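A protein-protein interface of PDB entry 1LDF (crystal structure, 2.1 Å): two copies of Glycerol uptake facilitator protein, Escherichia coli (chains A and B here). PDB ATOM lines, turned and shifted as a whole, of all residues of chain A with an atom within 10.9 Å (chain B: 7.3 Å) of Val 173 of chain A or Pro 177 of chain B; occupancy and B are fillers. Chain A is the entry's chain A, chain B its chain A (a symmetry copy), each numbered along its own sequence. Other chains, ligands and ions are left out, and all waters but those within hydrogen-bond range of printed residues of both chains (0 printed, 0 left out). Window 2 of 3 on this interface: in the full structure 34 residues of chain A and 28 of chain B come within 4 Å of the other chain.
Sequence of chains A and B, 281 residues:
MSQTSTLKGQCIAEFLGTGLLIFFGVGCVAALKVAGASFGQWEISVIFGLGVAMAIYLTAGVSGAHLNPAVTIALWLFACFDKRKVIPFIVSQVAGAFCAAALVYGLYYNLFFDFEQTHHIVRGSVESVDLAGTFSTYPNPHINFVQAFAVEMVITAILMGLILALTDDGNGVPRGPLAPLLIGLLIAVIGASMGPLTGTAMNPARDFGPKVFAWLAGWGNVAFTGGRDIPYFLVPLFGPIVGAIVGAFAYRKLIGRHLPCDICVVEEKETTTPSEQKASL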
ATOM      1  N   LEU A 164      18.665  14.250  -4.848  1.00  0.00           N
ATOM      2  CA  LEU A 164      17.467  15.068  -4.675  1.00  0.00           C
ATOM      3  C   LEU A 164      17.327  15.472  -3.209  1.00  0.00           C
ATOM      4  O   LEU A 164      16.986  16.616  -2.896  1.00  0.00           O
ATOM      5  CB  LEU A 164      16.217  14.302  -5.122  1.00  0.00           C
ATOM      6  CG  LEU A 164      16.143  13.963  -6.612  1.00  0.00           C
ATOM      7  CD1 LEU A 164      14.897  13.144  -6.890  1.00  0.00           C
ATOM      8  CD2 LEU A 164      16.138  15.246  -7.431  1.00  0.00           C
ATOM      9  N   ALA A 165      17.606  14.527  -2.317  1.00  0.00           N
ATOM     10  CA  ALA A 165      17.526  14.766  -0.883  1.00  0.00           C
ATOM     11  C   ALA A 165      18.521  15.831  -0.430  1.00  0.00           C
ATOM     12  O   ALA A 165      18.179  16.715   0.360  1.00  0.00           O
ATOM     13  CB  ALA A 165      17.782  13.471  -0.133  1.00  0.00           C
ATOM     14  N   LEU A 166      19.751  15.743  -0.930  1.00  0.00           N
ATOM     15  CA  LEU A 166      20.800  16.694  -0.564  1.00  0.00           C
ATOM     16  C   LEU A 166      20.578  18.091  -1.155  1.00  0.00           C
ATOM     17  O   LEU A 166      21.075  19.078  -0.617  1.00  0.00           O
ATOM     18  CB  LEU A 166      22.174  16.155  -0.998  1.00  0.00           C
ATOM     19  CG  LEU A 166      22.713  14.916  -0.262  1.00  0.00           C
ATOM     20  CD1 LEU A 166      23.934  14.386  -0.990  1.00  0.00           C
ATOM     21  CD2 LEU A 166      23.062  15.263   1.180  1.00  0.00           C
ATOM     22  N   THR A 167      19.840  18.173  -2.260  1.00  0.00           N
ATOM     23  CA  THR A 167      19.575  19.465  -2.895  1.00  0.00           C
ATOM     24  C   THR A 167      18.152  19.979  -2.639  1.00  0.00           C
ATOM     25  O   THR A 167      17.769  21.032  -3.149  1.00  0.00           O
ATOM     26  CB  THR A 167      19.794  19.403  -4.427  1.00  0.00           C
ATOM     27  OG1 THR A 167      18.932  18.406  -4.997  1.00  0.00           O
ATOM     28  CG2 THR A 167      21.253  19.075  -4.748  1.00  0.00           C
ATOM     29  N   ASP A 168      17.379  19.236  -1.852  1.00  0.00           N
ATOM     30  CA  ASP A 168      15.996  19.607  -1.535  1.00  0.00           C
ATOM     31  C   ASP A 168      15.940  20.539  -0.325  1.00  0.00           C
ATOM     32  O   ASP A 168      16.039  20.086   0.819  1.00  0.00           O
ATOM     33  CB  ASP A 168      15.182  18.343  -1.248  1.00  0.00           C
ATOM     34  CG  ASP A 168      13.720  18.636  -0.969  1.00  0.00           C
ATOM     35  OD1 ASP A 168      13.380  19.815  -0.733  1.00  0.00           O
ATOM     36  OD2 ASP A 168      12.915  17.681  -0.977  1.00  0.00           O
ATOM     37  N   ASP A 169      15.774  21.836  -0.572  1.00  0.00           N
ATOM     38  CA  ASP A 169      15.733  22.800   0.527  1.00  0.00           C
ATOM     39  C   ASP A 169      14.533  22.663   1.457  1.00  0.00           C
ATOM     40  O   ASP A 169      14.454  23.348   2.476  1.00  0.00           O
ATOM     41  CB  ASP A 169      15.825  24.230  -0.005  1.00  0.00           C
ATOM     42  CG  ASP A 169      17.210  24.559  -0.534  1.00  0.00           C
ATOM     43  OD1 ASP A 169      18.205  24.147   0.108  1.00  0.00           O
ATOM     44  OD2 ASP A 169      17.308  25.232  -1.583  1.00  0.00           O
ATOM     45  N   GLY A 170      13.610  21.771   1.119  1.00  0.00           N
ATOM     46  CA  GLY A 170      12.454  21.558   1.970  1.00  0.00           C
ATOM     47  C   GLY A 170      12.655  20.357   2.884  1.00  0.00           C
ATOM     48  O   GLY A 170      11.745  19.964   3.618  1.00  0.00           O
ATOM     49  N   ASN A 171      13.854  19.773   2.844  1.00  0.00           N
ATOM     50  CA  ASN A 171      14.175  18.606   3.665  1.00  0.00           C
ATOM     51  C   ASN A 171      15.244  18.966   4.688  1.00  0.00           C
ATOM     52  O   ASN A 171      16.425  19.037   4.350  1.00  0.00           O
ATOM     53  CB  ASN A 171      14.698  17.464   2.785  1.00  0.00           C
ATOM     54  CG  ASN A 171      14.836  16.155   3.549  1.00  0.00           C
ATOM     55  OD1 ASN A 171      15.091  16.147   4.754  1.00  0.00           O
ATOM     56  ND2 ASN A 171      14.678  15.042   2.846  1.00  0.00           N
ATOM     57  N   GLY A 172      14.835  19.188   5.931  1.00  0.00           N
ATOM     58  CA  GLY A 172      15.796  19.539   6.961  1.00  0.00           C
ATOM     59  C   GLY A 172      16.487  20.856   6.663  1.00  0.00           C
ATOM     60  O   GLY A 172      16.016  21.632   5.834  1.00  0.00           O
ATOM     61  N   VAL A 173      17.608  21.107   7.332  1.00  0.00           N
ATOM     62  CA  VAL A 173      18.357  22.343   7.136  1.00  0.00           C
ATOM     63  C   VAL A 173      19.057  22.366   5.780  1.00  0.00           C
ATOM     64  O   VAL A 173      19.831  21.462   5.452  1.00  0.00           O
ATOM     65  CB  VAL A 173      19.420  22.529   8.238  1.00  0.00           C
ATOM     66  CG1 VAL A 173      20.045  23.908   8.128  1.00  0.00           C
ATOM     67  CG2 VAL A 173      18.791  22.332   9.606  1.00  0.00           C
ATOM     68  N   PRO A 174      18.789  23.405   4.970  1.00  0.00           N
ATOM     69  CA  PRO A 174      19.395  23.551   3.641  1.00  0.00           C
ATOM     70  C   PRO A 174      20.919  23.402   3.689  1.00  0.00           C
ATOM     71  O   PRO A 174      21.568  23.973   4.567  1.00  0.00           O
ATOM     72  CB  PRO A 174      18.960  24.958   3.223  1.00  0.00           C
ATOM     73  CG  PRO A 174      17.609  25.090   3.868  1.00  0.00           C
ATOM     74  CD  PRO A 174      17.853  24.515   5.247  1.00  0.00           C
ATOM     75  N   ARG A 175      21.483  22.639   2.751  1.00  0.00           N
ATOM     76  CA  ARG A 175      22.932  22.428   2.710  1.00  0.00           C
ATOM     77  C   ARG A 175      23.717  23.579   2.098  1.00  0.00           C
ATOM     78  O   ARG A 175      24.887  23.777   2.428  1.00  0.00           O
ATOM     79  CB  ARG A 175      23.290  21.144   1.939  1.00  0.00           C
ATOM     80  CG  ARG A 175      22.923  19.849   2.641  1.00  0.00           C
ATOM     81  CD  ARG A 175      21.505  19.451   2.314  1.00  0.00           C
ATOM     82  NE  ARG A 175      20.782  19.081   3.517  1.00  0.00           N
ATOM     83  CZ  ARG A 175      19.472  18.886   3.566  1.00  0.00           C
ATOM     84  NH1 ARG A 175      18.738  19.022   2.467  1.00  0.00           N
ATOM     85  NH2 ARG A 175      18.901  18.569   4.717  1.00  0.00           N
ATOM     86  N   GLY A 176      23.092  24.328   1.196  1.00  0.00           N
ATOM     87  CA  GLY A 176      23.796  25.429   0.561  1.00  0.00           C
ATOM     88  C   GLY A 176      25.041  24.972  -0.189  1.00  0.00           C
ATOM     89  O   GLY A 176      24.979  24.019  -0.967  1.00  0.00           O
ATOM     90  N   PRO A 177      26.197  25.618   0.036  1.00  0.00           N
ATOM     91  CA  PRO A 177      27.450  25.267  -0.638  1.00  0.00           C
ATOM     92  C   PRO A 177      28.046  23.896  -0.290  1.00  0.00           C
ATOM     93  O   PRO A 177      29.015  23.467  -0.912  1.00  0.00           O
ATOM     94  CB  PRO A 177      28.374  26.421  -0.257  1.00  0.00           C
ATOM     95  CG  PRO A 177      27.923  26.748   1.135  1.00  0.00           C
ATOM     96  CD  PRO A 177      26.411  26.710   1.007  1.00  0.00           C
ATOM     97  N   LEU A 178      27.469  23.218   0.700  1.00  0.00           N
ATOM     98  CA  LEU A 178      27.934  21.896   1.114  1.00  0.00           C
ATOM     99  C   LEU A 178      27.413  20.793   0.198  1.00  0.00           C
ATOM    100  O   LEU A 178      27.999  19.709   0.124  1.00  0.00           O
ATOM    101  CB  LEU A 178      27.460  21.576   2.534  1.00  0.00           C
ATOM    102  CG  LEU A 178      28.231  22.041   3.766  1.00  0.00           C
ATOM    103  CD1 LEU A 178      27.414  21.706   5.010  1.00  0.00           C
ATOM    104  CD2 LEU A 178      29.591  21.360   3.823  1.00  0.00           C
ATOM    105  N   ALA A 179      26.308  21.073  -0.488  1.00  0.00           N
ATOM    106  CA  ALA A 179      25.672  20.100  -1.364  1.00  0.00           C
ATOM    107  C   ALA A 179      26.607  19.347  -2.321  1.00  0.00           C
ATOM    108  O   ALA A 179      26.665  18.120  -2.292  1.00  0.00           O
ATOM    109  CB  ALA A 179      24.529  20.772  -2.146  1.00  0.00           C
ATOM    110  N   PRO A 180      27.340  20.067  -3.187  1.00  0.00           N
ATOM    111  CA  PRO A 180      28.244  19.370  -4.116  1.00  0.00           C
ATOM    112  C   PRO A 180      29.237  18.446  -3.395  1.00  0.00           C
ATOM    113  O   PRO A 180      29.440  17.306  -3.810  1.00  0.00           O
ATOM    114  CB  PRO A 180      28.940  20.515  -4.847  1.00  0.00           C
ATOM    115  CG  PRO A 180      27.876  21.602  -4.846  1.00  0.00           C
ATOM    116  CD  PRO A 180      27.348  21.520  -3.431  1.00  0.00           C
ATOM    117  N   LEU A 181      29.844  18.944  -2.317  1.00  0.00           N
ATOM    118  CA  LEU A 181      30.804  18.166  -1.541  1.00  0.00           C
ATOM    119  C   LEU A 181      30.147  16.892  -1.031  1.00  0.00           C
ATOM    120  O   LEU A 181      30.698  15.799  -1.181  1.00  0.00           O
ATOM    121  CB  LEU A 181      31.324  18.975  -0.349  1.00  0.00           C
ATOM    122  CG  LEU A 181      32.232  18.217   0.637  1.00  0.00           C
ATOM    123  CD1 LEU A 181      33.519  17.775  -0.067  1.00  0.00           C
ATOM    124  CD2 LEU A 181      32.567  19.105   1.825  1.00  0.00           C
ATOM    125  N   LEU A 182      28.964  17.038  -0.441  1.00  0.00           N
ATOM    126  CA  LEU A 182      28.230  15.898   0.089  1.00  0.00           C
ATOM    127  C   LEU A 182      27.885  14.896  -1.009  1.00  0.00           C
ATOM    128  O   LEU A 182      27.893  13.691  -0.771  1.00  0.00           O
ATOM    129  CB  LEU A 182      26.953  16.366   0.806  1.00  0.00           C
ATOM    130  CG  LEU A 182      27.170  17.251   2.047  1.00  0.00           C
ATOM    131  CD1 LEU A 182      25.827  17.707   2.620  1.00  0.00           C
ATOM    132  CD2 LEU A 182      27.949  16.473   3.105  1.00  0.00           C
ATOM    133  N   ILE A 183      27.578  15.386  -2.204  1.00  0.00           N
ATOM    134  CA  ILE A 183      27.254  14.498  -3.319  1.00  0.00           C
ATOM    135  C   ILE A 183      28.511  13.711  -3.711  1.00  0.00           C
ATOM    136  O   ILE A 183      28.429  12.559  -4.140  1.00  0.00           O
ATOM    137  CB  ILE A 183      26.752  15.293  -4.542  1.00  0.00           C
ATOM    138  CG1 ILE A 183      25.397  15.935  -4.213  1.00  0.00           C
ATOM    139  CG2 ILE A 183      26.641  14.373  -5.763  1.00  0.00           C
ATOM    140  CD1 ILE A 183      24.911  16.929  -5.252  1.00  0.00           C
ATOM    141  N   LEU A 185      30.962  12.913  -1.593  1.00  0.00           N
ATOM    142  CA  LEU A 185      31.186  11.937  -0.529  1.00  0.00           C
ATOM    143  C   LEU A 185      30.232  10.761  -0.707  1.00  0.00           C
ATOM    144  O   LEU A 185      30.578   9.611  -0.394  1.00  0.00           O
ATOM    145  CB  LEU A 185      31.002  12.582   0.848  1.00  0.00           C
ATOM    146  CG  LEU A 185      32.117  13.557   1.245  1.00  0.00           C
ATOM    147  CD1 LEU A 185      31.855  14.058   2.660  1.00  0.00           C
ATOM    148  CD2 LEU A 185      33.495  12.866   1.169  1.00  0.00           C
ATOM    149  N   TYR A 251      12.042   8.819  -4.273  1.00  0.00           N
ATOM    150  CA  TYR A 251      12.256   9.958  -3.391  1.00  0.00           C
ATOM    151  C   TYR A 251      10.988  10.797  -3.219  1.00  0.00           C
ATOM    152  O   TYR A 251      10.585  11.108  -2.099  1.00  0.00           O
ATOM    153  CB  TYR A 251      13.371  10.865  -3.914  1.00  0.00           C
ATOM    154  CG  TYR A 251      13.624  12.043  -2.999  1.00  0.00           C
ATOM    155  CD1 TYR A 251      14.266  11.867  -1.774  1.00  0.00           C
ATOM    156  CD2 TYR A 251      13.151  13.318  -3.317  1.00  0.00           C
ATOM    157  CE1 TYR A 251      14.427  12.920  -0.886  1.00  0.00           C
ATOM    158  CE2 TYR A 251      13.306  14.388  -2.430  1.00  0.00           C
ATOM    159  CZ  TYR A 251      13.946  14.177  -1.216  1.00  0.00           C
ATOM    160  OH  TYR A 251      14.098  15.216  -0.326  1.00  0.00           O
ATOM    161  N   LEU A 259       7.167  15.646   3.365  1.00  0.00           N
ATOM    162  CA  LEU A 259       7.885  16.833   3.812  1.00  0.00           C
ATOM    163  C   LEU A 259       6.953  18.039   3.781  1.00  0.00           C
ATOM    164  O   LEU A 259       6.995  18.847   4.736  1.00  0.00           O
ATOM    165  CB  LEU A 259       9.103  17.091   2.916  1.00  0.00           C
ATOM    166  CG  LEU A 259      10.312  16.169   3.114  1.00  0.00           C
ATOM    167  CD1 LEU A 259      11.340  16.432   2.027  1.00  0.00           C
ATOM    168  CD2 LEU A 259      10.918  16.401   4.489  1.00  0.00           C
ATOM    169  N   TYR B  57      20.858  12.850   6.348  1.00  0.00           N
ATOM    170  CA  TYR B  57      20.462  13.913   5.433  1.00  0.00           C
ATOM    171  C   TYR B  57      19.176  13.531   4.705  1.00  0.00           C
ATOM    172  O   TYR B  57      18.325  14.380   4.421  1.00  0.00           O
ATOM    173  CB  TYR B  57      21.560  14.168   4.395  1.00  0.00           C
ATOM    174  CG  TYR B  57      22.716  14.987   4.907  1.00  0.00           C
ATOM    175  CD1 TYR B  57      22.513  16.286   5.380  1.00  0.00           C
ATOM    176  CD2 TYR B  57      24.016  14.472   4.920  1.00  0.00           C
ATOM    177  CE1 TYR B  57      23.571  17.050   5.851  1.00  0.00           C
ATOM    178  CE2 TYR B  57      25.083  15.230   5.390  1.00  0.00           C
ATOM    179  CZ  TYR B  57      24.852  16.519   5.856  1.00  0.00           C
ATOM    180  OH  TYR B  57      25.890  17.278   6.344  1.00  0.00           O
ATOM    181  N   ALA B  60      16.288  13.177   8.080  1.00  0.00           N
ATOM    182  CA  ALA B  60      16.149  14.146   9.163  1.00  0.00           C
ATOM    183  C   ALA B  60      14.860  14.965   9.082  1.00  0.00           C
ATOM    184  O   ALA B  60      14.137  15.096  10.069  1.00  0.00           O
ATOM    185  CB  ALA B  60      17.358  15.080   9.188  1.00  0.00           C
ATOM    186  N   GLY B  61      14.577  15.508   7.903  1.00  0.00           N
ATOM    187  CA  GLY B  61      13.392  16.327   7.721  1.00  0.00           C
ATOM    188  C   GLY B  61      12.056  15.649   7.949  1.00  0.00           C
ATOM    189  O   GLY B  61      11.048  16.327   8.171  1.00  0.00           O
ATOM    190  N   PRO B 174      26.033  27.241  16.302  1.00  0.00           N
ATOM    191  CA  PRO B 174      25.169  26.223  15.690  1.00  0.00           C
ATOM    192  C   PRO B 174      25.814  25.598  14.450  1.00  0.00           C
ATOM    193  O   PRO B 174      26.362  26.314  13.611  1.00  0.00           O
ATOM    194  CB  PRO B 174      23.902  27.013  15.354  1.00  0.00           C
ATOM    195  CG  PRO B 174      23.841  28.027  16.461  1.00  0.00           C
ATOM    196  CD  PRO B 174      25.281  28.488  16.555  1.00  0.00           C
ATOM    197  N   ARG B 175      25.748  24.270  14.337  1.00  0.00           N
ATOM    198  CA  ARG B 175      26.337  23.572  13.192  1.00  0.00           C
ATOM    199  C   ARG B 175      25.491  23.617  11.927  1.00  0.00           C
ATOM    200  O   ARG B 175      26.025  23.535  10.820  1.00  0.00           O
ATOM    201  CB  ARG B 175      26.622  22.096  13.521  1.00  0.00           C
ATOM    202  CG  ARG B 175      27.762  21.864  14.498  1.00  0.00           C
ATOM    203  CD  ARG B 175      27.260  21.910  15.920  1.00  0.00           C
ATOM    204  NE  ARG B 175      28.118  22.742  16.743  1.00  0.00           N
ATOM    205  CZ  ARG B 175      27.816  23.131  17.973  1.00  0.00           C
ATOM    206  NH1 ARG B 175      26.669  22.755  18.527  1.00  0.00           N
ATOM    207  NH2 ARG B 175      28.658  23.907  18.638  1.00  0.00           N
ATOM    208  N   GLY B 176      24.176  23.728  12.081  1.00  0.00           N
ATOM    209  CA  GLY B 176      23.314  23.755  10.911  1.00  0.00           C
ATOM    210  C   GLY B 176      23.446  22.499  10.058  1.00  0.00           C
ATOM    211  O   GLY B 176      23.393  21.387  10.583  1.00  0.00           O
ATOM    212  N   PRO B 177      23.640  22.642   8.736  1.00  0.00           N
ATOM    213  CA  PRO B 177      23.771  21.502   7.823  1.00  0.00           C
ATOM    214  C   PRO B 177      25.021  20.631   8.003  1.00  0.00           C
ATOM    215  O   PRO B 177      25.137  19.580   7.375  1.00  0.00           O
ATOM    216  CB  PRO B 177      23.710  22.163   6.448  1.00  0.00           C
ATOM    217  CG  PRO B 177      24.402  23.470   6.688  1.00  0.00           C
ATOM    218  CD  PRO B 177      23.809  23.918   8.012  1.00  0.00           C
ATOM    219  N   LEU B 178      25.947  21.067   8.853  1.00  0.00           N
ATOM    220  CA  LEU B 178      27.174  20.319   9.121  1.00  0.00           C
ATOM    221  C   LEU B 178      26.946  19.185  10.117  1.00  0.00           C
ATOM    222  O   LEU B 178      27.715  18.221  10.156  1.00  0.00           O
ATOM    223  CB  LEU B 178      28.250  21.235   9.707  1.00  0.00           C
ATOM    224  CG  LEU B 178      29.164  22.076   8.820  1.00  0.00           C
ATOM    225  CD1 LEU B 178      30.001  22.993   9.708  1.00  0.00           C
ATOM    226  CD2 LEU B 178      30.065  21.173   7.989  1.00  0.00           C
ATOM    227  N   ALA B 179      25.897  19.315  10.924  1.00  0.00           N
ATOM    228  CA  ALA B 179      25.585  18.335  11.955  1.00  0.00           C
ATOM    229  C   ALA B 179      25.627  16.865  11.515  1.00  0.00           C
ATOM    230  O   ALA B 179      26.372  16.070  12.084  1.00  0.00           O
ATOM    231  CB  ALA B 179      24.225  18.667  12.595  1.00  0.00           C
ATOM    232  N   PRO B 180      24.822  16.481  10.511  1.00  0.00           N
ATOM    233  CA  PRO B 180      24.842  15.076  10.071  1.00  0.00           C
ATOM    234  C   PRO B 180      26.249  14.596   9.686  1.00  0.00           C
ATOM    235  O   PRO B 180      26.664  13.507  10.080  1.00  0.00           O
ATOM    236  CB  PRO B 180      23.880  15.070   8.886  1.00  0.00           C
ATOM    237  CG  PRO B 180      22.892  16.165   9.257  1.00  0.00           C
ATOM    238  CD  PRO B 180      23.809  17.253   9.769  1.00  0.00           C
ATOM    239  N   LEU B 181      26.973  15.414   8.922  1.00  0.00           N
ATOM    240  CA  LEU B 181      28.327  15.077   8.493  1.00  0.00           C
ATOM    241  C   LEU B 181      29.211  14.837   9.708  1.00  0.00           C
ATOM    242  O   LEU B 181      29.916  13.828   9.781  1.00  0.00           O
ATOM    243  CB  LEU B 181      28.928  16.205   7.649  1.00  0.00           C
ATOM    244  CG  LEU B 181      30.407  16.040   7.257  1.00  0.00           C
ATOM    245  CD1 LEU B 181      30.579  14.810   6.360  1.00  0.00           C
ATOM    246  CD2 LEU B 181      30.896  17.284   6.533  1.00  0.00           C
ATOM    247  N   LEU B 182      29.159  15.762  10.663  1.00  0.00           N
ATOM    248  CA  LEU B 182      29.955  15.650  11.876  1.00  0.00           C
ATOM    249  C   LEU B 182      29.596  14.396  12.668  1.00  0.00           C
ATOM    250  O   LEU B 182      30.465  13.774  13.270  1.00  0.00           O
ATOM    251  CB  LEU B 182      29.781  16.902  12.751  1.00  0.00           C
ATOM    252  CG  LEU B 182      30.270  18.224  12.131  1.00  0.00           C
ATOM    253  CD1 LEU B 182      29.973  19.396  13.067  1.00  0.00           C
ATOM    254  CD2 LEU B 182      31.771  18.142  11.861  1.00  0.00           C
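N of Gly 61 of chain B sits at hydrogen-bond distance from OD1 of Asn 171 of chain A, 3.3 Å away.
NH1 of Arg 175 of chain A sits at hydrogen-bond distance from O of Ala 165 of chain A (3.2 Å). The backbone carbonyl oxygen of Asp 168 of chain A sits at hydrogen-bond distance from the guanidinium group of Arg 175 of chain A (3.3 Å). O of Asn 171 of chain A lies within hydrogen-bond range of NH2 of Arg 175 of chain A (2.5 Å). The side-chain amide nitrogen (ND2) of Asn 171 of chain A lies within hydrogen-bond range of the side-chain hydroxyl (OH) of Tyr 251 of chain A (3.2 Å). O of Val 173 of chain A is in hydrogen-bond range of NH2 of Arg 175 of chain A. The side-chain hydroxyl (OH) of Tyr 57 of chain B lies within hydrogen-bond range of the backbone carbonyl oxygen (O) of Pro 177 of chain B (2.6 Å).
Among the printed residues, merely in contact across the chains: Pro 174 of chain A with Pro 177 of chain B, Leu 182 of chain A with Tyr 57 of chain B, Gly 172 of chain A with Gly 61 of chain B, Leu 259 of chain A with Gly 61 of chain B, Asn 171 of chain A with Tyr 57 of chain B, Leu 166 of chain A with Tyr 57 of chain B, Val 173 of chain A with Pro 177 of chain B, Arg 175 of chain A with Tyr 57 of chain B, Arg 175 of chain A with Pro 177 of chain B, Leu 178 of chain A with Pro 177 of chain B and Leu 185 of chain A with Leu 181 of chain B.
Of chain B, only Pro 177 comes within 4 Å of Val 173 of chain A. No residue of chain A comes within 4 Å of Gly 176 of chain B. No residue of chain A comes within 4 Å of Leu 178 of chain B. No residue of chain A comes within 4 Å of Pro 180 of chain B. Of the printed residues of chain A, Leu 181 of chain B touches Leu 185 (3.99 Å). Printed residues of chain B within 4 Å of Leu 182 of chain A: Tyr 57. Printed residues of chain A within 4 Å of Gly 61 of chain B: Asn 171 (3.3 Å), Gly 172 (3.7 Å) and Leu 259 (3.7 Å). Ala 60 of chain B touches none of the printed residues of chain A. Asp 168 of chain A touches none of the printed residues of chain B. The nearest residue of chain B that does not touch Val 173 of chain A is Gly 176 of chain B (4.2 Å). The nearest residue of chain A that does not touch Pro 177 of chain B is Leu 182 of chain A (5.2 Å). The nearest printed residue of chain B that does not touch Asn 171 of chain A is Ala 60 of chain B (4.5 Å).
Of the 12 printed residues of chain B, 4 touch a printed residue of chain A. Printed residues of chain B that touch a printed residue of chain A: Tyr 57, Gly 61, Pro 177 and Leu 181. Of the 23 printed residues of chain A, 10 touch a printed residue of chain B.
Pro 174 of chain A touches Pro 177 of chain B, but with the chains exchanged Pro 177 of chain A does not touch Pro 174 of chain B (12.6 Å). Arg 175 of chain A touches Pro 177 of chain B, but with the chains exchanged Pro 177 of chain A does not touch Arg 175 of chain B (10.3 Å). Leu 178 of chain A touches Pro 177 of chain B, but with the chains exchanged Pro 177 of chain A does not touch Leu 178 of chain B (8.9 Å). Of the 12 pairs that touch across the chains among the printed residues, none has its exchanged pair printed and touching as well.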
